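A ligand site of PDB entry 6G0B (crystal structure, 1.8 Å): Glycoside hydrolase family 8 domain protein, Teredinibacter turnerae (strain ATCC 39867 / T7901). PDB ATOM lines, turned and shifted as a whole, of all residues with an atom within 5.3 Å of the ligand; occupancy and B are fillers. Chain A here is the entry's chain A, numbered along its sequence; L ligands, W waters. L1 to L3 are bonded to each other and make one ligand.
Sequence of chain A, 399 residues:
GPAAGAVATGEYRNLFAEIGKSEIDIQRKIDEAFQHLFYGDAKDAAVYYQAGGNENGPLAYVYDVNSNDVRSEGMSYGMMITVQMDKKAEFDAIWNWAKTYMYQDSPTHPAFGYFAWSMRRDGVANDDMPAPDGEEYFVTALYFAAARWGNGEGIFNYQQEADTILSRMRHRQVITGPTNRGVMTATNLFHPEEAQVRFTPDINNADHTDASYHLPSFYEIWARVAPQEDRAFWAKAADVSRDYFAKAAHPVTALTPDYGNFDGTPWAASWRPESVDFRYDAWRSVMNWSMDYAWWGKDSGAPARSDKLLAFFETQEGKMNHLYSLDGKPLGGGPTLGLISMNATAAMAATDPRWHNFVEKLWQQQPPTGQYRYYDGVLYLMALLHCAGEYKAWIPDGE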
ATOM      1  N   ARG A  71      19.474  10.910  15.151  1.00  0.00           N
ATOM      2  CA  ARG A  71      20.255   9.822  14.563  1.00  0.00           C
ATOM      3  C   ARG A  71      20.800  10.213  13.218  1.00  0.00           C
ATOM      4  O   ARG A  71      20.148  10.977  12.472  1.00  0.00           O
ATOM      5  CB  ARG A  71      19.416   8.575  14.480  1.00  0.00           C
ATOM      6  CG  ARG A  71      19.064   8.089  15.891  1.00  0.00           C
ATOM      7  CD  ARG A  71      18.324   6.772  15.898  1.00  0.00           C
ATOM      8  NE  ARG A  71      18.217   6.220  17.240  1.00  0.00           N
ATOM      9  CZ  ARG A  71      17.621   5.069  17.520  1.00  0.00           C
ATOM     10  NH1 ARG A  71      17.082   4.356  16.518  1.00  0.00           N
ATOM     11  NH2 ARG A  71      17.593   4.617  18.777  1.00  0.00           N
ATOM     12  N   SER A  72      21.950   9.652  12.866  1.00  0.00           N
ATOM     13  CA  SER A  72      22.531   9.876  11.514  1.00  0.00           C
ATOM     14  C   SER A  72      21.591   9.387  10.427  1.00  0.00           C
ATOM     15  O   SER A  72      21.457  10.026   9.380  1.00  0.00           O
ATOM     16  CB  SER A  72      23.910   9.254  11.402  1.00  0.00           C
ATOM     17  OG  SER A  72      23.882   7.841  11.494  1.00  0.00           O
ATOM     18  N   GLU A  73      20.872   8.298  10.705  1.00  0.00           N
ATOM     19  CA  GLU A  73      19.795   7.827   9.803  1.00  0.00           C
ATOM     20  C   GLU A  73      18.807   8.944   9.438  1.00  0.00           C
ATOM     21  O   GLU A  73      18.548   9.198   8.258  1.00  0.00           O
ATOM     22  CB  GLU A  73      19.028   6.678  10.461  1.00  0.00           C
ATOM     23  CG  GLU A  73      17.717   6.266   9.812  1.00  0.00           C
ATOM     24  CD  GLU A  73      16.843   5.436  10.741  1.00  0.00           C
ATOM     25  OE1 GLU A  73      16.216   6.011  11.667  1.00  0.00           O
ATOM     26  OE2 GLU A  73      16.793   4.200  10.534  1.00  0.00           O
ATOM     27  N   TRP A 117      26.441   8.081  15.263  1.00  0.00           N
ATOM     28  CA  TRP A 117      25.084   7.668  14.880  1.00  0.00           C
ATOM     29  C   TRP A 117      23.941   8.163  15.775  1.00  0.00           C
ATOM     30  O   TRP A 117      22.813   8.263  15.285  1.00  0.00           O
ATOM     31  CB  TRP A 117      24.990   6.159  14.758  1.00  0.00           C
ATOM     32  CG  TRP A 117      24.762   5.383  16.049  1.00  0.00           C
ATOM     33  CD1 TRP A 117      25.708   4.873  16.909  1.00  0.00           C
ATOM     34  CD2 TRP A 117      23.511   5.009  16.600  1.00  0.00           C
ATOM     35  NE1 TRP A 117      25.109   4.203  17.924  1.00  0.00           N
ATOM     36  CE2 TRP A 117      23.761   4.284  17.782  1.00  0.00           C
ATOM     37  CE3 TRP A 117      22.190   5.230  16.216  1.00  0.00           C
ATOM     38  CZ2 TRP A 117      22.738   3.754  18.575  1.00  0.00           C
ATOM     39  CZ3 TRP A 117      21.184   4.713  16.997  1.00  0.00           C
ATOM     40  CH2 TRP A 117      21.463   4.003  18.185  1.00  0.00           C
ATOM     41  N   ASP A 127      26.927   8.004  21.170  1.00  0.00           N
ATOM     42  CA  ASP A 127      27.826   6.981  20.670  1.00  0.00           C
ATOM     43  C   ASP A 127      28.597   7.585  19.516  1.00  0.00           C
ATOM     44  O   ASP A 127      27.983   8.014  18.543  1.00  0.00           O
ATOM     45  CB  ASP A 127      27.007   5.738  20.231  1.00  0.00           C
ATOM     46  CG  ASP A 127      27.880   4.566  19.804  1.00  0.00           C
ATOM     47  OD1 ASP A 127      29.134   4.721  19.708  1.00  0.00           O
ATOM     48  OD2 ASP A 127      27.317   3.464  19.557  1.00  0.00           O
ATOM     49  N   MET A 129      30.578   6.081  17.438  1.00  0.00           N
ATOM     50  CA  MET A 129      30.646   5.192  16.274  1.00  0.00           C
ATOM     51  C   MET A 129      29.511   5.502  15.288  1.00  0.00           C
ATOM     52  O   MET A 129      28.438   5.945  15.705  1.00  0.00           O
ATOM     53  CB  MET A 129      30.480   3.710  16.635  1.00  0.00           C
ATOM     54  CG  MET A 129      31.616   3.066  17.403  1.00  0.00           C
ATOM     55  SD  MET A 129      33.118   2.897  16.387  1.00  0.00           S
ATOM     56  CE  MET A 129      33.955   4.356  17.041  1.00  0.00           C
ATOM     57  N   PRO A 130      29.728   5.175  14.008  1.00  0.00           N
ATOM     58  CA  PRO A 130      28.712   5.424  12.995  1.00  0.00           C
ATOM     59  C   PRO A 130      27.764   4.285  12.786  1.00  0.00           C
ATOM     60  O   PRO A 130      28.034   3.161  13.205  1.00  0.00           O
ATOM     61  CB  PRO A 130      29.560   5.625  11.739  1.00  0.00           C
ATOM     62  CG  PRO A 130      30.657   4.616  11.944  1.00  0.00           C
ATOM     63  CD  PRO A 130      31.011   4.799  13.393  1.00  0.00           C
ATOM     64  N   ALA A 131      26.630   4.604  12.174  1.00  0.00           N
ATOM     65  CA  ALA A 131      25.711   3.595  11.626  1.00  0.00           C
ATOM     66  C   ALA A 131      25.823   3.727  10.109  1.00  0.00           C
ATOM     67  O   ALA A 131      25.382   4.750   9.539  1.00  0.00           O
ATOM     68  CB  ALA A 131      24.284   3.840  12.079  1.00  0.00           C
ATOM     69  N   ASP A 133      24.470   2.918   7.331  1.00  0.00           N
ATOM     70  CA  ASP A 133      23.371   3.369   6.455  1.00  0.00           C
ATOM     71  C   ASP A 133      23.228   4.909   6.405  1.00  0.00           C
ATOM     72  O   ASP A 133      22.838   5.468   5.361  1.00  0.00           O
ATOM     73  CB  ASP A 133      22.033   2.687   6.771  1.00  0.00           C
ATOM     74  CG  ASP A 133      21.508   2.947   8.159  1.00  0.00           C
ATOM     75  OD1 ASP A 133      22.297   3.098   9.127  1.00  0.00           O
ATOM     76  OD2 ASP A 133      20.261   2.941   8.308  1.00  0.00           O
ATOM     77  N   GLY A 134      23.516   5.577   7.534  1.00  0.00           N
ATOM     78  CA  GLY A 134      23.621   7.036   7.576  1.00  0.00           C
ATOM     79  C   GLY A 134      24.575   7.536   6.506  1.00  0.00           C
ATOM     80  O   GLY A 134      24.192   8.287   5.620  1.00  0.00           O
ATOM     81  N   ARG A 181      32.988   6.396  24.711  1.00  0.00           N
ATOM     82  CA  ARG A 181      32.705   5.117  25.336  1.00  0.00           C
ATOM     83  C   ARG A 181      33.949   4.422  25.910  1.00  0.00           C
ATOM     84  O   ARG A 181      33.848   3.335  26.432  1.00  0.00           O
ATOM     85  CB  ARG A 181      31.962   4.194  24.356  1.00  0.00           C
ATOM     86  CG  ARG A 181      30.564   4.714  24.066  1.00  0.00           C
ATOM     87  CD  ARG A 181      29.899   4.112  22.837  1.00  0.00           C
ATOM     88  NE  ARG A 181      29.888   2.651  22.926  1.00  0.00           N
ATOM     89  CZ  ARG A 181      30.016   1.804  21.919  1.00  0.00           C
ATOM     90  NH1 ARG A 181      30.177   2.194  20.635  1.00  0.00           N
ATOM     91  NH2 ARG A 181      30.035   0.524  22.217  1.00  0.00           N
ATOM     92  N   MET A 184      38.390   2.390  21.797  1.00  0.00           N
ATOM     93  CA  MET A 184      37.788   1.514  20.804  1.00  0.00           C
ATOM     94  C   MET A 184      38.660   1.394  19.552  1.00  0.00           C
ATOM     95  O   MET A 184      39.528   2.204  19.271  1.00  0.00           O
ATOM     96  CB  MET A 184      36.393   2.027  20.392  1.00  0.00           C
ATOM     97  CG  MET A 184      35.441   2.194  21.547  1.00  0.00           C
ATOM     98  SD  MET A 184      33.718   2.457  21.076  1.00  0.00           S
ATOM     99  CE  MET A 184      33.419   0.912  20.240  1.00  0.00           C
ATOM    100  N   PHE A 199      27.644  -3.732   9.286  1.00  0.00           N
ATOM    101  CA  PHE A 199      26.740  -3.250  10.356  1.00  0.00           C
ATOM    102  C   PHE A 199      27.465  -2.202  11.246  1.00  0.00           C
ATOM    103  O   PHE A 199      26.872  -1.223  11.638  1.00  0.00           O
ATOM    104  CB  PHE A 199      26.226  -4.424  11.180  1.00  0.00           C
ATOM    105  CG  PHE A 199      25.493  -3.988  12.423  1.00  0.00           C
ATOM    106  CD1 PHE A 199      24.184  -3.547  12.329  1.00  0.00           C
ATOM    107  CD2 PHE A 199      26.135  -3.943  13.648  1.00  0.00           C
ATOM    108  CE1 PHE A 199      23.530  -3.064  13.460  1.00  0.00           C
ATOM    109  CE2 PHE A 199      25.464  -3.490  14.788  1.00  0.00           C
ATOM    110  CZ  PHE A 199      24.169  -3.061  14.685  1.00  0.00           C
ATOM    111  N   THR A 200      28.746  -2.403  11.541  1.00  0.00           N
ATOM    112  CA  THR A 200      29.522  -1.459  12.345  1.00  0.00           C
ATOM    113  C   THR A 200      30.973  -1.585  11.964  1.00  0.00           C
ATOM    114  O   THR A 200      31.378  -2.699  11.571  1.00  0.00           O
ATOM    115  CB  THR A 200      29.376  -1.732  13.870  1.00  0.00           C
ATOM    116  OG1 THR A 200      30.131  -0.782  14.589  1.00  0.00           O
ATOM    117  CG2 THR A 200      29.868  -3.111  14.281  1.00  0.00           C
ATOM    118  N   ASP A 202      33.172  -1.057  14.234  1.00  0.00           N
ATOM    119  CA  ASP A 202      33.719  -1.523  15.506  1.00  0.00           C
ATOM    120  C   ASP A 202      34.238  -2.955  15.283  1.00  0.00           C
ATOM    121  O   ASP A 202      33.477  -3.852  14.894  1.00  0.00           O
ATOM    122  CB  ASP A 202      32.649  -1.469  16.610  1.00  0.00           C
ATOM    123  CG  ASP A 202      33.115  -2.035  17.967  1.00  0.00           C
ATOM    124  OD1 ASP A 202      34.250  -2.556  18.106  1.00  0.00           O
ATOM    125  OD2 ASP A 202      32.254  -1.979  18.906  1.00  0.00           O
ATOM    126  N   ASN A 204      35.011  -5.313  17.169  1.00  0.00           N
ATOM    127  CA  ASN A 204      34.301  -6.384  17.890  1.00  0.00           C
ATOM    128  C   ASN A 204      33.124  -7.010  17.156  1.00  0.00           C
ATOM    129  O   ASN A 204      32.806  -8.159  17.430  1.00  0.00           O
ATOM    130  CB  ASN A 204      33.843  -5.910  19.280  1.00  0.00           C
ATOM    131  CG  ASN A 204      35.013  -5.668  20.207  1.00  0.00           C
ATOM    132  OD1 ASN A 204      36.041  -6.359  20.135  1.00  0.00           O
ATOM    133  ND2 ASN A 204      34.872  -4.694  21.083  1.00  0.00           N
ATOM    134  N   ASN A 205      32.464  -6.273  16.250  1.00  0.00           N
ATOM    135  CA  ASN A 205      31.313  -6.832  15.519  1.00  0.00           C
ATOM    136  C   ASN A 205      31.354  -6.479  14.044  1.00  0.00           C
ATOM    137  O   ASN A 205      30.303  -6.405  13.394  1.00  0.00           O
ATOM    138  CB  ASN A 205      30.026  -6.312  16.153  1.00  0.00           C
ATOM    139  CG  ASN A 205      29.763  -6.890  17.527  1.00  0.00           C
ATOM    140  OD1 ASN A 205      29.493  -8.077  17.652  1.00  0.00           O
ATOM    141  ND2 ASN A 205      29.782  -6.070  18.533  1.00  0.00           N
ATOM    142  N   SER A 212      18.878  -4.265   5.123  1.00  0.00           N
ATOM    143  CA  SER A 212      18.366  -2.906   4.907  1.00  0.00           C
ATOM    144  C   SER A 212      19.424  -1.839   4.637  1.00  0.00           C
ATOM    145  O   SER A 212      19.075  -0.737   4.210  1.00  0.00           O
ATOM    146  CB  SER A 212      17.497  -2.456   6.096  1.00  0.00           C
ATOM    147  OG  SER A 212      18.271  -2.046   7.216  1.00  0.00           O
ATOM    148  N   TYR A 213      20.701  -2.117   4.909  1.00  0.00           N
ATOM    149  CA  TYR A 213      21.782  -1.210   4.578  1.00  0.00           C
ATOM    150  C   TYR A 213      22.287  -1.418   3.140  1.00  0.00           C
ATOM    151  O   TYR A 213      23.064  -0.641   2.663  1.00  0.00           O
ATOM    152  CB  TYR A 213      22.969  -1.399   5.497  1.00  0.00           C
ATOM    153  CG  TYR A 213      22.806  -1.058   6.961  1.00  0.00           C
ATOM    154  CD1 TYR A 213      21.554  -0.794   7.537  1.00  0.00           C
ATOM    155  CD2 TYR A 213      23.928  -1.037   7.766  1.00  0.00           C
ATOM    156  CE1 TYR A 213      21.465  -0.472   8.892  1.00  0.00           C
ATOM    157  CE2 TYR A 213      23.845  -0.727   9.123  1.00  0.00           C
ATOM    158  CZ  TYR A 213      22.616  -0.456   9.683  1.00  0.00           C
ATOM    159  OH  TYR A 213      22.553  -0.189  11.014  1.00  0.00           O
ATOM    160  N   TYR A 259      19.419  -8.043  11.007  1.00  0.00           N
ATOM    161  CA  TYR A 259      20.875  -8.126  10.918  1.00  0.00           C
ATOM    162  C   TYR A 259      21.254  -9.429  10.265  1.00  0.00           C
ATOM    163  O   TYR A 259      20.497 -10.404  10.364  1.00  0.00           O
ATOM    164  CB  TYR A 259      21.582  -8.079  12.288  1.00  0.00           C
ATOM    165  CG  TYR A 259      21.344  -6.880  13.163  1.00  0.00           C
ATOM    166  CD1 TYR A 259      20.780  -5.711  12.666  1.00  0.00           C
ATOM    167  CD2 TYR A 259      21.721  -6.916  14.489  1.00  0.00           C
ATOM    168  CE1 TYR A 259      20.550  -4.625  13.512  1.00  0.00           C
ATOM    169  CE2 TYR A 259      21.512  -5.845  15.338  1.00  0.00           C
ATOM    170  CZ  TYR A 259      20.935  -4.708  14.863  1.00  0.00           C
ATOM    171  OH  TYR A 259      20.723  -3.651  15.726  1.00  0.00           O
ATOM    172  N   TRP A 271      23.581  -8.583  22.057  1.00  0.00           N
ATOM    173  CA  TRP A 271      22.841  -7.627  22.850  1.00  0.00           C
ATOM    174  C   TRP A 271      21.398  -7.479  22.338  1.00  0.00           C
ATOM    175  O   TRP A 271      20.617  -6.740  22.927  1.00  0.00           O
ATOM    176  CB  TRP A 271      23.522  -6.261  22.825  1.00  0.00           C
ATOM    177  CG  TRP A 271      23.523  -5.634  21.469  1.00  0.00           C
ATOM    178  CD1 TRP A 271      22.599  -4.794  20.958  1.00  0.00           C
ATOM    179  CD2 TRP A 271      24.481  -5.845  20.444  1.00  0.00           C
ATOM    180  NE1 TRP A 271      22.911  -4.467  19.679  1.00  0.00           N
ATOM    181  CE2 TRP A 271      24.075  -5.107  19.335  1.00  0.00           C
ATOM    182  CE3 TRP A 271      25.654  -6.606  20.354  1.00  0.00           C
ATOM    183  CZ2 TRP A 271      24.804  -5.076  18.143  1.00  0.00           C
ATOM    184  CZ3 TRP A 271      26.367  -6.588  19.173  1.00  0.00           C
ATOM    185  CH2 TRP A 271      25.917  -5.861  18.075  1.00  0.00           C
ATOM    186  N   ASP A 281      14.274  -2.515  11.083  1.00  0.00           N
ATOM    187  CA  ASP A 281      15.248  -2.309  10.001  1.00  0.00           C
ATOM    188  C   ASP A 281      14.793  -2.962   8.698  1.00  0.00           C
ATOM    189  O   ASP A 281      14.839  -2.340   7.621  1.00  0.00           O
ATOM    190  CB  ASP A 281      16.595  -2.919  10.318  1.00  0.00           C
ATOM    191  CG  ASP A 281      17.440  -2.041  11.226  1.00  0.00           C
ATOM    192  OD1 ASP A 281      16.896  -1.283  12.037  1.00  0.00           O
ATOM    193  OD2 ASP A 281      18.683  -2.151  11.100  1.00  0.00           O
ATOM    194  N   ARG A 284      12.588  -2.007   5.425  1.00  0.00           N
ATOM    195  CA  ARG A 284      13.133  -1.182   4.359  1.00  0.00           C
ATOM    196  C   ARG A 284      13.748  -1.969   3.224  1.00  0.00           C
ATOM    197  O   ARG A 284      13.938  -1.406   2.157  1.00  0.00           O
ATOM    198  CB  ARG A 284      14.183  -0.213   4.918  1.00  0.00           C
ATOM    199  CG  ARG A 284      13.661   0.606   6.074  1.00  0.00           C
ATOM    200  CD  ARG A 284      14.730   1.486   6.660  1.00  0.00           C
ATOM    201  NE  ARG A 284      15.757   0.645   7.291  1.00  0.00           N
ATOM    202  CZ  ARG A 284      16.622   1.057   8.196  1.00  0.00           C
ATOM    203  NH1 ARG A 284      16.614   2.327   8.604  1.00  0.00           N
ATOM    204  NH2 ARG A 284      17.500   0.191   8.730  1.00  0.00           N
ATOM    205  N   TYR A 375       9.986   7.531  12.885  1.00  0.00           N
ATOM    206  CA  TYR A 375      10.348   6.461  12.007  1.00  0.00           C
ATOM    207  C   TYR A 375       9.209   6.251  11.001  1.00  0.00           C
ATOM    208  O   TYR A 375       9.435   6.200   9.779  1.00  0.00           O
ATOM    209  CB  TYR A 375      10.686   5.182  12.771  1.00  0.00           C
ATOM    210  CG  TYR A 375      11.413   4.161  11.922  1.00  0.00           C
ATOM    211  CD1 TYR A 375      12.580   4.495  11.240  1.00  0.00           C
ATOM    212  CD2 TYR A 375      10.925   2.876  11.774  1.00  0.00           C
ATOM    213  CE1 TYR A 375      13.248   3.560  10.484  1.00  0.00           C
ATOM    214  CE2 TYR A 375      11.582   1.925  11.043  1.00  0.00           C
ATOM    215  CZ  TYR A 375      12.734   2.262  10.378  1.00  0.00           C
ATOM    216  OH  TYR A 375      13.362   1.313   9.644  1.00  0.00           O
HETATM  217  O1  LIG L   1      17.048   1.666  12.463  1.00  0.00           O
HETATM  218  C1  LIG L   1      18.461   1.520  12.767  1.00  0.00           C
HETATM  219  C2  LIG L   1      19.250   2.389  11.791  1.00  0.00           C
HETATM  220  C3  LIG L   1      20.738   2.534  12.150  1.00  0.00           C
HETATM  221  C4  LIG L   1      21.045   2.633  13.649  1.00  0.00           C
HETATM  222  C5  LIG L   1      19.744   2.901  14.367  1.00  0.00           C
HETATM  223  O2  LIG L   1      19.086   1.865  10.457  1.00  0.00           O
HETATM  224  O3  LIG L   1      21.178   3.737  11.532  1.00  0.00           O
HETATM  225  O4  LIG L   1      21.622   1.419  14.130  1.00  0.00           O
HETATM  226  O5  LIG L   1      18.786   1.863  14.131  1.00  0.00           O
HETATM  227  C1  LG2 L   2      22.542   1.459  15.196  1.00  0.00           C
HETATM  228  C2  LG2 L   2      22.388   0.237  16.093  1.00  0.00           C
HETATM  229  C3  LG2 L   2      23.432   0.273  17.205  1.00  0.00           C
HETATM  230  C4  LG2 L   2      24.823   0.341  16.578  1.00  0.00           C
HETATM  231  C5  LG2 L   2      24.916   1.436  15.538  1.00  0.00           C
HETATM  232  O1  LG2 L   2      21.090   0.166  16.646  1.00  0.00           O
HETATM  233  O2  LG2 L   2      23.378  -0.928  17.966  1.00  0.00           O
HETATM  234  O3  LG2 L   2      25.795   0.550  17.611  1.00  0.00           O
HETATM  235  O4  LG2 L   2      23.825   1.400  14.620  1.00  0.00           O
HETATM  236  C1  LG3 L   3      26.920  -0.278  17.457  1.00  0.00           C
HETATM  237  C2  LG3 L   3      28.042   0.220  18.353  1.00  0.00           C
HETATM  238  C3  LG3 L   3      29.224  -0.700  18.200  1.00  0.00           C
HETATM  239  C4  LG3 L   3      28.822  -2.131  18.527  1.00  0.00           C
HETATM  240  C5  LG3 L   3      27.560  -2.527  17.757  1.00  0.00           C
HETATM  241  O1  LG3 L   3      28.387   1.580  18.043  1.00  0.00           O
HETATM  242  O2  LG3 L   3      30.176  -0.225  19.143  1.00  0.00           O
HETATM  243  O3  LG3 L   3      29.885  -3.055  18.189  1.00  0.00           O
HETATM  244  O4  LG3 L   3      26.498  -1.583  17.869  1.00  0.00           O
HETATM  245  O   HOH W   1      21.654   6.361  12.698  1.00  0.00           O
HETATM  246  O   HOH W   2      19.812  -1.474  14.923  1.00  0.00           O
HETATM  247  O   HOH W   3      20.089   1.030  19.191  1.00  0.00           O
HETATM  248  O   HOH W   4      28.714   1.431  15.162  1.00  0.00           O
HETATM  249  O   HOH W   5      24.646   0.299  12.262  1.00  0.00           O
HETATM  250  O   HOH W   6      16.844   1.167  15.753  1.00  0.00           O
HETATM  251  O   HOH W   7      21.234  -2.843  18.147  1.00  0.00           O
HETATM  252  O   HOH W   8      24.329  -0.535  20.499  1.00  0.00           O
HETATM  253  O   HOH W   9      20.449  -1.142  12.557  1.00  0.00           O
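NH1 of Arg 181 lies within salt-bridge range of OD1 of Asp 127 (2.9 Å).
The backbone NH of Asp 202 lies within hydrogen-bond range of the side-chain hydroxyl of Thr 200, 3.1 Å away.
NH2 of Arg 284 is in salt-bridge range of OD2 of Asp 281, 3.5 Å away.
OE2 of Glu 73 lies within salt-bridge range of NH1 of Arg 284 (2.7 Å).
The side-chain hydroxyl of Tyr 375 lies close to the guanidinium group of Arg 284 (3.4 Å).
The side-chain hydroxyl of Ser 212 is in hydrogen-bond range of the guanidinium group of Arg 284, 2.8 Å away.
O of Asp 281 lies close to OG of Ser 212 (3.5 Å).
The backbone carbonyl oxygen (O) of Met 129 sits at hydrogen-bond distance from the backbone NH (N) of Trp 117, at 3.0 Å.
NH1 of Arg 71 touches C5 of LIG L1, at 3.7 Å.
CZ3 of Trp 117 touches C5 of LIG L1 (3.5 Å).
CB of Met 129 touches O1 of LG3 L3, at 3.3 Å.
CB of Ala 131 touches O3 of LIG L1, 3.2 Å away.
CE of Met 184 touches O2 of LG3 L3, at 3.6 Å.
CE2 of Phe 199 touches C5 of LG3 L3, 3.8 Å away.
OG1 of Thr 200 touches C3 of LG3 L3, at 3.7 Å.
Tyr 213 touches the ligand.
OH of Tyr 259 touches O1 of LG2 L2, 3.9 Å away.
Trp 271 touches the ligand.
Within 4 Å of the ligand: Arg 71, Glu 73, Trp 117, Asp 127, Met 129, Ala 131, Asp 133, Arg 181, Met 184, Phe 199, Thr 200, Asp 202, Asn 205, Tyr 213, Tyr 259, Trp 271, Asp 281 and Arg 284.
OD2 of Asp 127 is in hydrogen-bond range of O1 of LG3 L3, at 2.6 Å.
OD2 of Asp 133 lies within hydrogen-bond range of O2 of LIG L1 (2.7 Å).
OD2 of Asp 202 lies within hydrogen-bond range of O3 of LG3 L3.
An oxygen (O2) of LG3 L3 sits at hydrogen-bond distance from the guanidinium group (NH1) of Arg 181 (2.8 Å).
An oxygen (O2) of LIG L1 lies within hydrogen-bond range of the guanidinium group (NH2) of Arg 284.
An oxygen (O1) of LIG L1 is in hydrogen-bond range of the side-chain carboxylate (OD1) of Asp 281 (3.0 Å).
The side-chain amide nitrogen (ND2) of Asn 205 lies within hydrogen-bond range of an oxygen (O3) of LG3 L3 (3.0 Å).
An oxygen (O1) of LIG L1 is in hydrogen-bond range of the side-chain carboxylate (OE2) of Glu 73 (3.2 Å).
Water W6 lies within hydrogen-bond range of O5 of LIG L1 (2.6 Å) and NH1 of Arg 71 (3.3 Å).
Water W2 bridges the side-chain hydroxyl of Tyr 259 and an oxygen (O1) of LG2 L2.
Water W5 lies within hydrogen-bond range of OH of Tyr 213 (2.5 Å), O4 of LG2 L2 (2.7 Å) and O of Phe 199 (2.8 Å).
Water W7 lies within hydrogen-bond range of OH of Tyr 259 (2.6 Å), NE1 of Trp 271 (2.8 Å) and O2 of LG2 L2 (2.9 Å).
Water W4 lies within hydrogen-bond range of OG1 of Thr 200, O of Pro 130 and O1 of LG3 L3.
Water W9 lies within hydrogen-bond range of the side-chain carboxylate of Asp 281 (2.5 Å), the side-chain hydroxyl of Tyr 213 (2.8 Å) and an oxygen (O4) of LIG L1 (3.2 Å).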
